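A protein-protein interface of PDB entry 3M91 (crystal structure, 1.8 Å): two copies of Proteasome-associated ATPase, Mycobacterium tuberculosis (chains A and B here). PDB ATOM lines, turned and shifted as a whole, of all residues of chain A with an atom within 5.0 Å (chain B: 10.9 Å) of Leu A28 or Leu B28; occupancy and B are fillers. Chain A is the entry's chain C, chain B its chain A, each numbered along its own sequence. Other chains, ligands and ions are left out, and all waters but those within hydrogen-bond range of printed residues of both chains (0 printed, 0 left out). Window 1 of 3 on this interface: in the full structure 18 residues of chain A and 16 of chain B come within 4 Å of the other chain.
Of the 17 printed residues of chain B, 4 touch a printed residue of chain A.
Of the 9 printed residues of chain A, 5 touch a printed residue of chain B.
Hydrophobic or aromatic side chains of chain A that line the printed part of chain B: Leu A28 and Leu A32.
Along chain A the printed residues that touch a printed residue of chain B span positions 24 to 32.
Printed residues of chain B within 4 Å of Asn A25: Asn B25 and Leu B28.
No residue of chain B comes within 4 Å of Lys A27.
Printed residues of chain B within 4 Å of Leu A28: Asn B25, Leu B28 and Leu B32.
No residue of chain B comes within 4 Å of Met A29.
Of the printed residues of chain B, Thr A31 touches Leu B32 (3.9 Å).
Leu A32 touches three residues of chain B.
Ala B22 touches none of the printed residues of chain A.
Of the printed residues of chain A, Leu B28 touches Asn A25, Leu A28 and Leu A32.
Printed residues of chain A within 4 Å of Leu B32: Leu A28, Thr A31 and Leu A32.
The nearest printed residue of chain B that does not touch Leu A28 is Met B29 (4.3 Å).
The nearest printed residue of chain A that does not touch Leu B28 is Met A29 (4.2 Å).
ND2 of Asn B25 lies close to OD1 of Asn A25, 3.3 Å away.
Asn B25 touches its own counterpart, Asn A25.
Asn A25 touches Leu B28, and with the chains exchanged Leu A28 touches Asn B25.
Leu A28 touches its own counterpart, Leu B28.
Thr A31 touches Leu B32, and with the chains exchanged Leu A32 touches Thr B31.
Positions printed for both chains: 24, 25, 26, 27, 28, 29, 30, 31 and 32.
O of Lys A27 sits at hydrogen-bond distance from OG1 of Thr A31 (2.8 Å).
ND2 of Asn B25 sits close to O of Leu B21 (3.4 Å).
The backbone carbonyl oxygen of Lys B27 lies within hydrogen-bond range of the side-chain hydroxyl of Thr B31, at 2.7 Å.
Among the printed residues, merely in contact across the chains: Asn A25 with Leu B28, Arg A24 with Asn B25, Leu A32 with Leu B28, Leu A28 with Asn B25, Leu A28 with Leu B32, Thr A31 with Leu B32, Leu A28 with Leu B28, Leu A32 with Leu B32 and Leu A32 with Thr B31.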
ATOM      1  N   ARG A  24      19.922 -29.415   9.401  1.00  0.00           N
ATOM      2  CA  ARG A  24      19.112 -29.564  10.565  1.00  0.00           C
ATOM      3  C   ARG A  24      17.691 -29.095  10.288  1.00  0.00           C
ATOM      4  O   ARG A  24      16.765 -29.765  10.633  1.00  0.00           O
ATOM      5  CB  ARG A  24      19.687 -28.832  11.770  1.00  0.00           C
ATOM      6  CG  ARG A  24      20.925 -29.498  12.387  1.00  0.00           C
ATOM      7  CD  ARG A  24      21.458 -28.826  13.701  1.00  0.00           C
ATOM      8  NE  ARG A  24      22.648 -29.510  14.215  1.00  0.00           N
ATOM      9  CZ  ARG A  24      23.070 -29.480  15.477  1.00  0.00           C
ATOM     10  NH1 ARG A  24      22.417 -28.799  16.391  1.00  0.00           N
ATOM     11  NH2 ARG A  24      24.168 -30.129  15.832  1.00  0.00           N
ATOM     12  N   ASN A  25      17.537 -27.980   9.614  1.00  0.00           N
ATOM     13  CA  ASN A  25      16.223 -27.465   9.310  1.00  0.00           C
ATOM     14  C   ASN A  25      15.440 -28.366   8.390  1.00  0.00           C
ATOM     15  O   ASN A  25      14.280 -28.572   8.593  1.00  0.00           O
ATOM     16  CB  ASN A  25      16.437 -26.102   8.430  1.00  0.00           C
ATOM     17  CG  ASN A  25      15.107 -25.438   7.889  1.00  0.00           C
ATOM     18  OD1 ASN A  25      14.511 -24.594   8.563  1.00  0.00           O
ATOM     19  ND2 ASN A  25      14.712 -25.759   6.647  1.00  0.00           N
ATOM     20  N   SER A  26      16.090 -28.887   7.376  1.00  0.00           N
ATOM     21  CA  SER A  26      15.544 -29.840   6.476  1.00  0.00           C
ATOM     22  C   SER A  26      15.044 -31.057   7.265  1.00  0.00           C
ATOM     23  O   SER A  26      13.940 -31.493   7.034  1.00  0.00           O
ATOM     24  CB  SER A  26      16.605 -30.262   5.511  1.00  0.00           C
ATOM     25  OG  SER A  26      16.054 -31.168   4.579  1.00  0.00           O
ATOM     26  N   LYS A  27      15.838 -31.576   8.193  1.00  0.00           N
ATOM     27  CA  LYS A  27      15.411 -32.761   8.961  1.00  0.00           C
ATOM     28  C   LYS A  27      14.195 -32.414   9.858  1.00  0.00           C
ATOM     29  O   LYS A  27      13.250 -33.211  10.015  1.00  0.00           O
ATOM     30  CB  LYS A  27      16.567 -33.245   9.823  1.00  0.00           C
ATOM     31  CG  LYS A  27      16.244 -34.467  10.644  1.00  0.00           C
ATOM     32  CD  LYS A  27      16.141 -35.696   9.717  1.00  0.00           C
ATOM     33  CE  LYS A  27      15.779 -36.995  10.474  1.00  0.00           C
ATOM     34  NZ  LYS A  27      14.821 -37.884   9.711  1.00  0.00           N
ATOM     35  N   LEU A  28      14.233 -31.235  10.474  1.00  0.00           N
ATOM     36  CA  LEU A  28      13.162 -30.833  11.343  1.00  0.00           C
ATOM     37  C   LEU A  28      11.883 -30.687  10.551  1.00  0.00           C
ATOM     38  O   LEU A  28      10.801 -30.978  11.077  1.00  0.00           O
ATOM     39  CB  LEU A  28      13.478 -29.504  12.028  1.00  0.00           C
ATOM     40  CG  LEU A  28      14.428 -29.596  13.233  1.00  0.00           C
ATOM     41  CD1 LEU A  28      14.860 -28.180  13.680  1.00  0.00           C
ATOM     42  CD2 LEU A  28      13.916 -30.369  14.490  1.00  0.00           C
ATOM     43  N   MET A  29      11.992 -30.183   9.324  1.00  0.00           N
ATOM     44  CA  MET A  29      10.830 -29.889   8.491  1.00  0.00           C
ATOM     45  C   MET A  29      10.188 -31.167   8.005  1.00  0.00           C
ATOM     46  O   MET A  29       8.951 -31.298   7.983  1.00  0.00           O
ATOM     47  CB  MET A  29      11.255 -29.063   7.271  1.00  0.00           C
ATOM     48  CG  MET A  29      10.082 -28.455   6.599  1.00  0.00           C
ATOM     49  SD  MET A  29      10.461 -27.044   5.471  1.00  0.00           S
ATOM     50  CE  MET A  29      11.739 -26.209   6.398  1.00  0.00           C
ATOM     51  N   GLU A  30      11.019 -32.104   7.586  1.00  0.00           N
ATOM     52  CA  GLU A  30      10.548 -33.419   7.229  1.00  0.00           C
ATOM     53  C   GLU A  30       9.819 -34.141   8.384  1.00  0.00           C
ATOM     54  O   GLU A  30       8.753 -34.813   8.151  1.00  0.00           O
ATOM     55  CB  GLU A  30      11.716 -34.305   6.735  1.00  0.00           C
ATOM     56  CG  GLU A  30      11.283 -35.720   6.202  1.00  0.00           C
ATOM     57  CD  GLU A  30      10.019 -35.673   5.218  1.00  0.00           C
ATOM     58  OE1 GLU A  30      10.124 -34.996   4.134  1.00  0.00           O
ATOM     59  OE2 GLU A  30       8.925 -36.315   5.534  1.00  0.00           O
ATOM     60  N   THR A  31      10.405 -34.051   9.582  1.00  0.00           N
ATOM     61  CA  THR A  31       9.825 -34.710  10.757  1.00  0.00           C
ATOM     62  C   THR A  31       8.502 -34.031  11.088  1.00  0.00           C
ATOM     63  O   THR A  31       7.540 -34.700  11.490  1.00  0.00           O
ATOM     64  CB  THR A  31      10.745 -34.614  11.978  1.00  0.00           C
ATOM     65  OG1 THR A  31      12.020 -35.125  11.577  1.00  0.00           O
ATOM     66  CG2 THR A  31      10.234 -35.509  13.067  1.00  0.00           C
ATOM     67  N   LEU A  32       8.447 -32.705  10.957  1.00  0.00           N
ATOM     68  CA  LEU A  32       7.206 -32.046  11.252  1.00  0.00           C
ATOM     69  C   LEU A  32       6.075 -32.396  10.225  1.00  0.00           C
ATOM     70  O   LEU A  32       4.882 -32.486  10.585  1.00  0.00           O
ATOM     71  CB  LEU A  32       7.506 -30.518  11.340  1.00  0.00           C
ATOM     72  CG  LEU A  32       6.447 -29.590  11.902  1.00  0.00           C
ATOM     73  CD1 LEU A  32       6.004 -29.971  13.322  1.00  0.00           C
ATOM     74  CD2 LEU A  32       6.944 -28.090  11.783  1.00  0.00           C
ATOM     75  N   SER B  20      19.186 -16.133  10.833  1.00  0.00           N
ATOM     76  CA  SER B  20      17.924 -16.487  10.206  1.00  0.00           C
ATOM     77  C   SER B  20      17.608 -17.980  10.355  1.00  0.00           C
ATOM     78  O   SER B  20      16.506 -18.333  10.804  1.00  0.00           O
ATOM     79  CB  SER B  20      17.912 -16.093   8.715  1.00  0.00           C
ATOM     80  OG  SER B  20      16.847 -16.762   8.014  1.00  0.00           O
ATOM     81  N   LEU B  21      18.560 -18.830   9.963  1.00  0.00           N
ATOM     82  CA  LEU B  21      18.425 -20.260  10.074  1.00  0.00           C
ATOM     83  C   LEU B  21      18.310 -20.694  11.526  1.00  0.00           C
ATOM     84  O   LEU B  21      17.497 -21.602  11.832  1.00  0.00           O
ATOM     85  CB  LEU B  21      19.526 -21.044   9.375  1.00  0.00           C
ATOM     86  CG  LEU B  21      19.664 -20.953   7.868  1.00  0.00           C
ATOM     87  CD1 LEU B  21      21.050 -21.484   7.536  1.00  0.00           C
ATOM     88  CD2 LEU B  21      18.637 -21.709   7.098  1.00  0.00           C
ATOM     89  N   ALA B  22      19.034 -20.025  12.409  1.00  0.00           N
ATOM     90  CA  ALA B  22      18.962 -20.314  13.831  1.00  0.00           C
ATOM     91  C   ALA B  22      17.556 -20.056  14.403  1.00  0.00           C
ATOM     92  O   ALA B  22      17.064 -20.859  15.210  1.00  0.00           O
ATOM     93  CB  ALA B  22      20.004 -19.535  14.602  1.00  0.00           C
ATOM     94  N   ALA B  23      16.934 -18.950  13.992  1.00  0.00           N
ATOM     95  CA  ALA B  23      15.553 -18.605  14.392  1.00  0.00           C
ATOM     96  C   ALA B  23      14.492 -19.598  13.830  1.00  0.00           C
ATOM     97  O   ALA B  23      13.586 -19.993  14.555  1.00  0.00           O
ATOM     98  CB  ALA B  23      15.199 -17.170  13.989  1.00  0.00           C
ATOM     99  N   ARG B  24      14.626 -19.950  12.548  1.00  0.00           N
ATOM    100  CA  ARG B  24      13.836 -20.950  11.901  1.00  0.00           C
ATOM    101  C   ARG B  24      13.945 -22.320  12.575  1.00  0.00           C
ATOM    102  O   ARG B  24      12.922 -22.968  12.806  1.00  0.00           O
ATOM    103  CB  ARG B  24      14.154 -21.052  10.419  1.00  0.00           C
ATOM    104  CG  ARG B  24      13.433 -19.963   9.595  1.00  0.00           C
ATOM    105  CD  ARG B  24      14.278 -19.423   8.393  1.00  0.00           C
ATOM    106  NE  ARG B  24      13.461 -19.156   7.194  1.00  0.00           N
ATOM    107  CZ  ARG B  24      13.657 -19.746   6.006  1.00  0.00           C
ATOM    108  NH1 ARG B  24      14.688 -20.606   5.858  1.00  0.00           N
ATOM    109  NH2 ARG B  24      12.840 -19.466   4.967  1.00  0.00           N
ATOM    110  N   ASN B  25      15.143 -22.728  12.921  1.00  0.00           N
ATOM    111  CA  ASN B  25      15.348 -23.973  13.613  1.00  0.00           C
ATOM    112  C   ASN B  25      14.673 -23.983  14.955  1.00  0.00           C
ATOM    113  O   ASN B  25      14.029 -24.929  15.291  1.00  0.00           O
ATOM    114  CB  ASN B  25      16.782 -24.228  13.493  1.00  0.00           C
ATOM    115  CG  ASN B  25      17.127 -25.048  12.301  1.00  0.00           C
ATOM    116  OD1 ASN B  25      17.971 -25.925  12.328  1.00  0.00           O
ATOM    117  ND2 ASN B  25      16.461 -24.755  11.223  1.00  0.00           N
ATOM    118  N   SER B  26      14.831 -22.922  15.714  1.00  0.00           N
ATOM    119  CA  SER B  26      14.168 -22.713  16.964  1.00  0.00           C
ATOM    120  C   SER B  26      12.641 -22.851  16.844  1.00  0.00           C
ATOM    121  O   SER B  26      12.033 -23.528  17.665  1.00  0.00           O
ATOM    122  CB  SER B  26      14.493 -21.338  17.455  1.00  0.00           C
ATOM    123  OG  SER B  26      13.993 -21.185  18.768  1.00  0.00           O
ATOM    124  N   LYS B  27      12.045 -22.235  15.822  1.00  0.00           N
ATOM    125  CA  LYS B  27      10.607 -22.298  15.614  1.00  0.00           C
ATOM    126  C   LYS B  27      10.161 -23.734  15.246  1.00  0.00           C
ATOM    127  O   LYS B  27       9.102 -24.221  15.714  1.00  0.00           O
ATOM    128  CB  LYS B  27      10.185 -21.311  14.525  1.00  0.00           C
ATOM    129  CG  LYS B  27       8.686 -21.253  14.251  1.00  0.00           C
ATOM    130  CD  LYS B  27       7.926 -20.611  15.457  1.00  0.00           C
ATOM    131  CE  LYS B  27       6.362 -20.760  15.387  1.00  0.00           C
ATOM    132  NZ  LYS B  27       5.650 -21.131  16.700  1.00  0.00           N
ATOM    133  N   LEU B  28      10.942 -24.403  14.410  1.00  0.00           N
ATOM    134  CA  LEU B  28      10.599 -25.717  13.983  1.00  0.00           C
ATOM    135  C   LEU B  28      10.666 -26.649  15.172  1.00  0.00           C
ATOM    136  O   LEU B  28       9.837 -27.563  15.283  1.00  0.00           O
ATOM    137  CB  LEU B  28      11.513 -26.235  12.865  1.00  0.00           C
ATOM    138  CG  LEU B  28      11.207 -25.669  11.457  1.00  0.00           C
ATOM    139  CD1 LEU B  28      12.406 -25.972  10.526  1.00  0.00           C
ATOM    140  CD2 LEU B  28       9.953 -26.188  10.806  1.00  0.00           C
ATOM    141  N   MET B  29      11.649 -26.437  16.029  1.00  0.00           N
ATOM    142  CA  MET B  29      11.882 -27.306  17.191  1.00  0.00           C
ATOM    143  C   MET B  29      10.777 -27.206  18.255  1.00  0.00           C
ATOM    144  O   MET B  29      10.323 -28.227  18.835  1.00  0.00           O
ATOM    145  CB  MET B  29      13.207 -26.958  17.853  1.00  0.00           C
ATOM    146  CG  MET B  29      13.685 -28.123  18.657  1.00  0.00           C
ATOM    147  SD  MET B  29      15.448 -28.101  19.193  1.00  0.00           S
ATOM    148  CE  MET B  29      16.260 -27.209  17.855  1.00  0.00           C
ATOM    149  N   GLU B  30      10.414 -25.964  18.553  1.00  0.00           N
ATOM    150  CA  GLU B  30       9.272 -25.658  19.367  1.00  0.00           C
ATOM    151  C   GLU B  30       7.962 -26.309  18.837  1.00  0.00           C
ATOM    152  O   GLU B  30       7.162 -26.858  19.649  1.00  0.00           O
ATOM    153  CB  GLU B  30       9.059 -24.136  19.503  1.00  0.00           C
ATOM    154  CG  GLU B  30       7.948 -23.708  20.540  1.00  0.00           C
ATOM    155  CD  GLU B  30       8.054 -24.464  21.939  1.00  0.00           C
ATOM    156  OE1 GLU B  30       9.149 -24.384  22.593  1.00  0.00           O
ATOM    157  OE2 GLU B  30       7.039 -25.154  22.371  1.00  0.00           O
ATOM    158  N   THR B  31       7.716 -26.165  17.531  1.00  0.00           N
ATOM    159  CA  THR B  31       6.485 -26.664  16.929  1.00  0.00           C
ATOM    160  C   THR B  31       6.510 -28.217  17.018  1.00  0.00           C
ATOM    161  O   THR B  31       5.496 -28.846  17.247  1.00  0.00           O
ATOM    162  CB  THR B  31       6.327 -26.209  15.474  1.00  0.00           C
ATOM    163  OG1 THR B  31       6.439 -24.775  15.456  1.00  0.00           O
ATOM    164  CG2 THR B  31       4.930 -26.536  15.001  1.00  0.00           C
ATOM    165  N   LEU B  32       7.673 -28.822  16.788  1.00  0.00           N
ATOM    166  CA  LEU B  32       7.778 -30.262  16.888  1.00  0.00           C
ATOM    167  C   LEU B  32       7.581 -30.789  18.359  1.00  0.00           C
ATOM    168  O   LEU B  32       6.960 -31.873  18.578  1.00  0.00           O
ATOM    169  CB  LEU B  32       9.152 -30.664  16.308  1.00  0.00           C
ATOM    170  CG  LEU B  32       9.371 -32.124  15.968  1.00  0.00           C
ATOM    171  CD1 LEU B  32       8.327 -32.773  14.991  1.00  0.00           C
ATOM    172  CD2 LEU B  32      10.829 -32.262  15.418  1.00  0.00           C
ATOM    173  N   LYS B  33       8.055 -30.038  19.353  1.00  0.00           N
ATOM    174  CA  LYS B  33       7.805 -30.411  20.755  1.00  0.00           C
ATOM    175  C   LYS B  33       6.291 -30.380  21.017  1.00  0.00           C
ATOM    176  O   LYS B  33       5.781 -31.251  21.682  1.00  0.00           O
ATOM    177  CB  LYS B  33       8.463 -29.452  21.695  1.00  0.00           C
ATOM    178  CG  LYS B  33       9.928 -29.823  21.946  1.00  0.00           C
ATOM    179  CD  LYS B  33      10.665 -28.719  22.774  1.00  0.00           C
ATOM    180  CE  LYS B  33      12.152 -29.105  22.902  1.00  0.00           C
ATOM    181  NZ  LYS B  33      13.043 -27.921  22.978  1.00  0.00           N
ATOM    182  N   GLU B  34       5.576 -29.349  20.522  1.00  0.00           N
ATOM    183  CA  GLU B  34       4.145 -29.311  20.600  1.00  0.00           C
ATOM    184  C   GLU B  34       3.494 -30.500  19.898  1.00  0.00           C
ATOM    185  O   GLU B  34       2.553 -31.068  20.458  1.00  0.00           O
ATOM    186  CB  GLU B  34       3.526 -28.003  20.063  1.00  0.00           C
ATOM    187  CG  GLU B  34       4.026 -26.791  20.925  1.00  0.00           C
ATOM    188  CD  GLU B  34       3.738 -25.398  20.268  1.00  0.00           C
ATOM    189  OE1 GLU B  34       3.100 -25.354  19.208  1.00  0.00           O
ATOM    190  OE2 GLU B  34       4.182 -24.354  20.833  1.00  0.00           O
ATOM    191  N   ALA B  35       3.981 -30.891  18.725  1.00  0.00           N
ATOM    192  CA  ALA B  35       3.365 -31.998  17.990  1.00  0.00           C
ATOM    193  C   ALA B  35       3.605 -33.291  18.754  1.00  0.00           C
ATOM    194  O   ALA B  35       2.703 -34.162  18.818  1.00  0.00           O
ATOM    195  CB  ALA B  35       3.996 -32.147  16.570  1.00  0.00           C
ATOM    196  N   ARG B  36       4.825 -33.440  19.317  1.00  0.00           N
ATOM    197  CA  ARG B  36       5.134 -34.588  20.191  1.00  0.00           C
ATOM    198  C   ARG B  36       4.095 -34.768  21.324  1.00  0.00           C
ATOM    199  O   ARG B  36       3.587 -35.883  21.458  1.00  0.00           O
ATOM    200  CB  ARG B  36       6.581 -34.465  20.748  1.00  0.00           C
ATOM    201  CG  ARG B  36       7.195 -35.861  21.074  1.00  0.00           C
ATOM    202  CD  ARG B  36       7.089 -36.165  22.534  1.00  0.00           C
ATOM    203  NE  ARG B  36       7.787 -37.435  22.879  1.00  0.00           N
ATOM    204  CZ  ARG B  36       7.310 -38.407  23.687  1.00  0.00           C
ATOM    205  NH1 ARG B  36       6.115 -38.316  24.303  1.00  0.00           N
ATOM    206  NH2 ARG B  36       8.002 -39.531  23.823  1.00  0.00           N
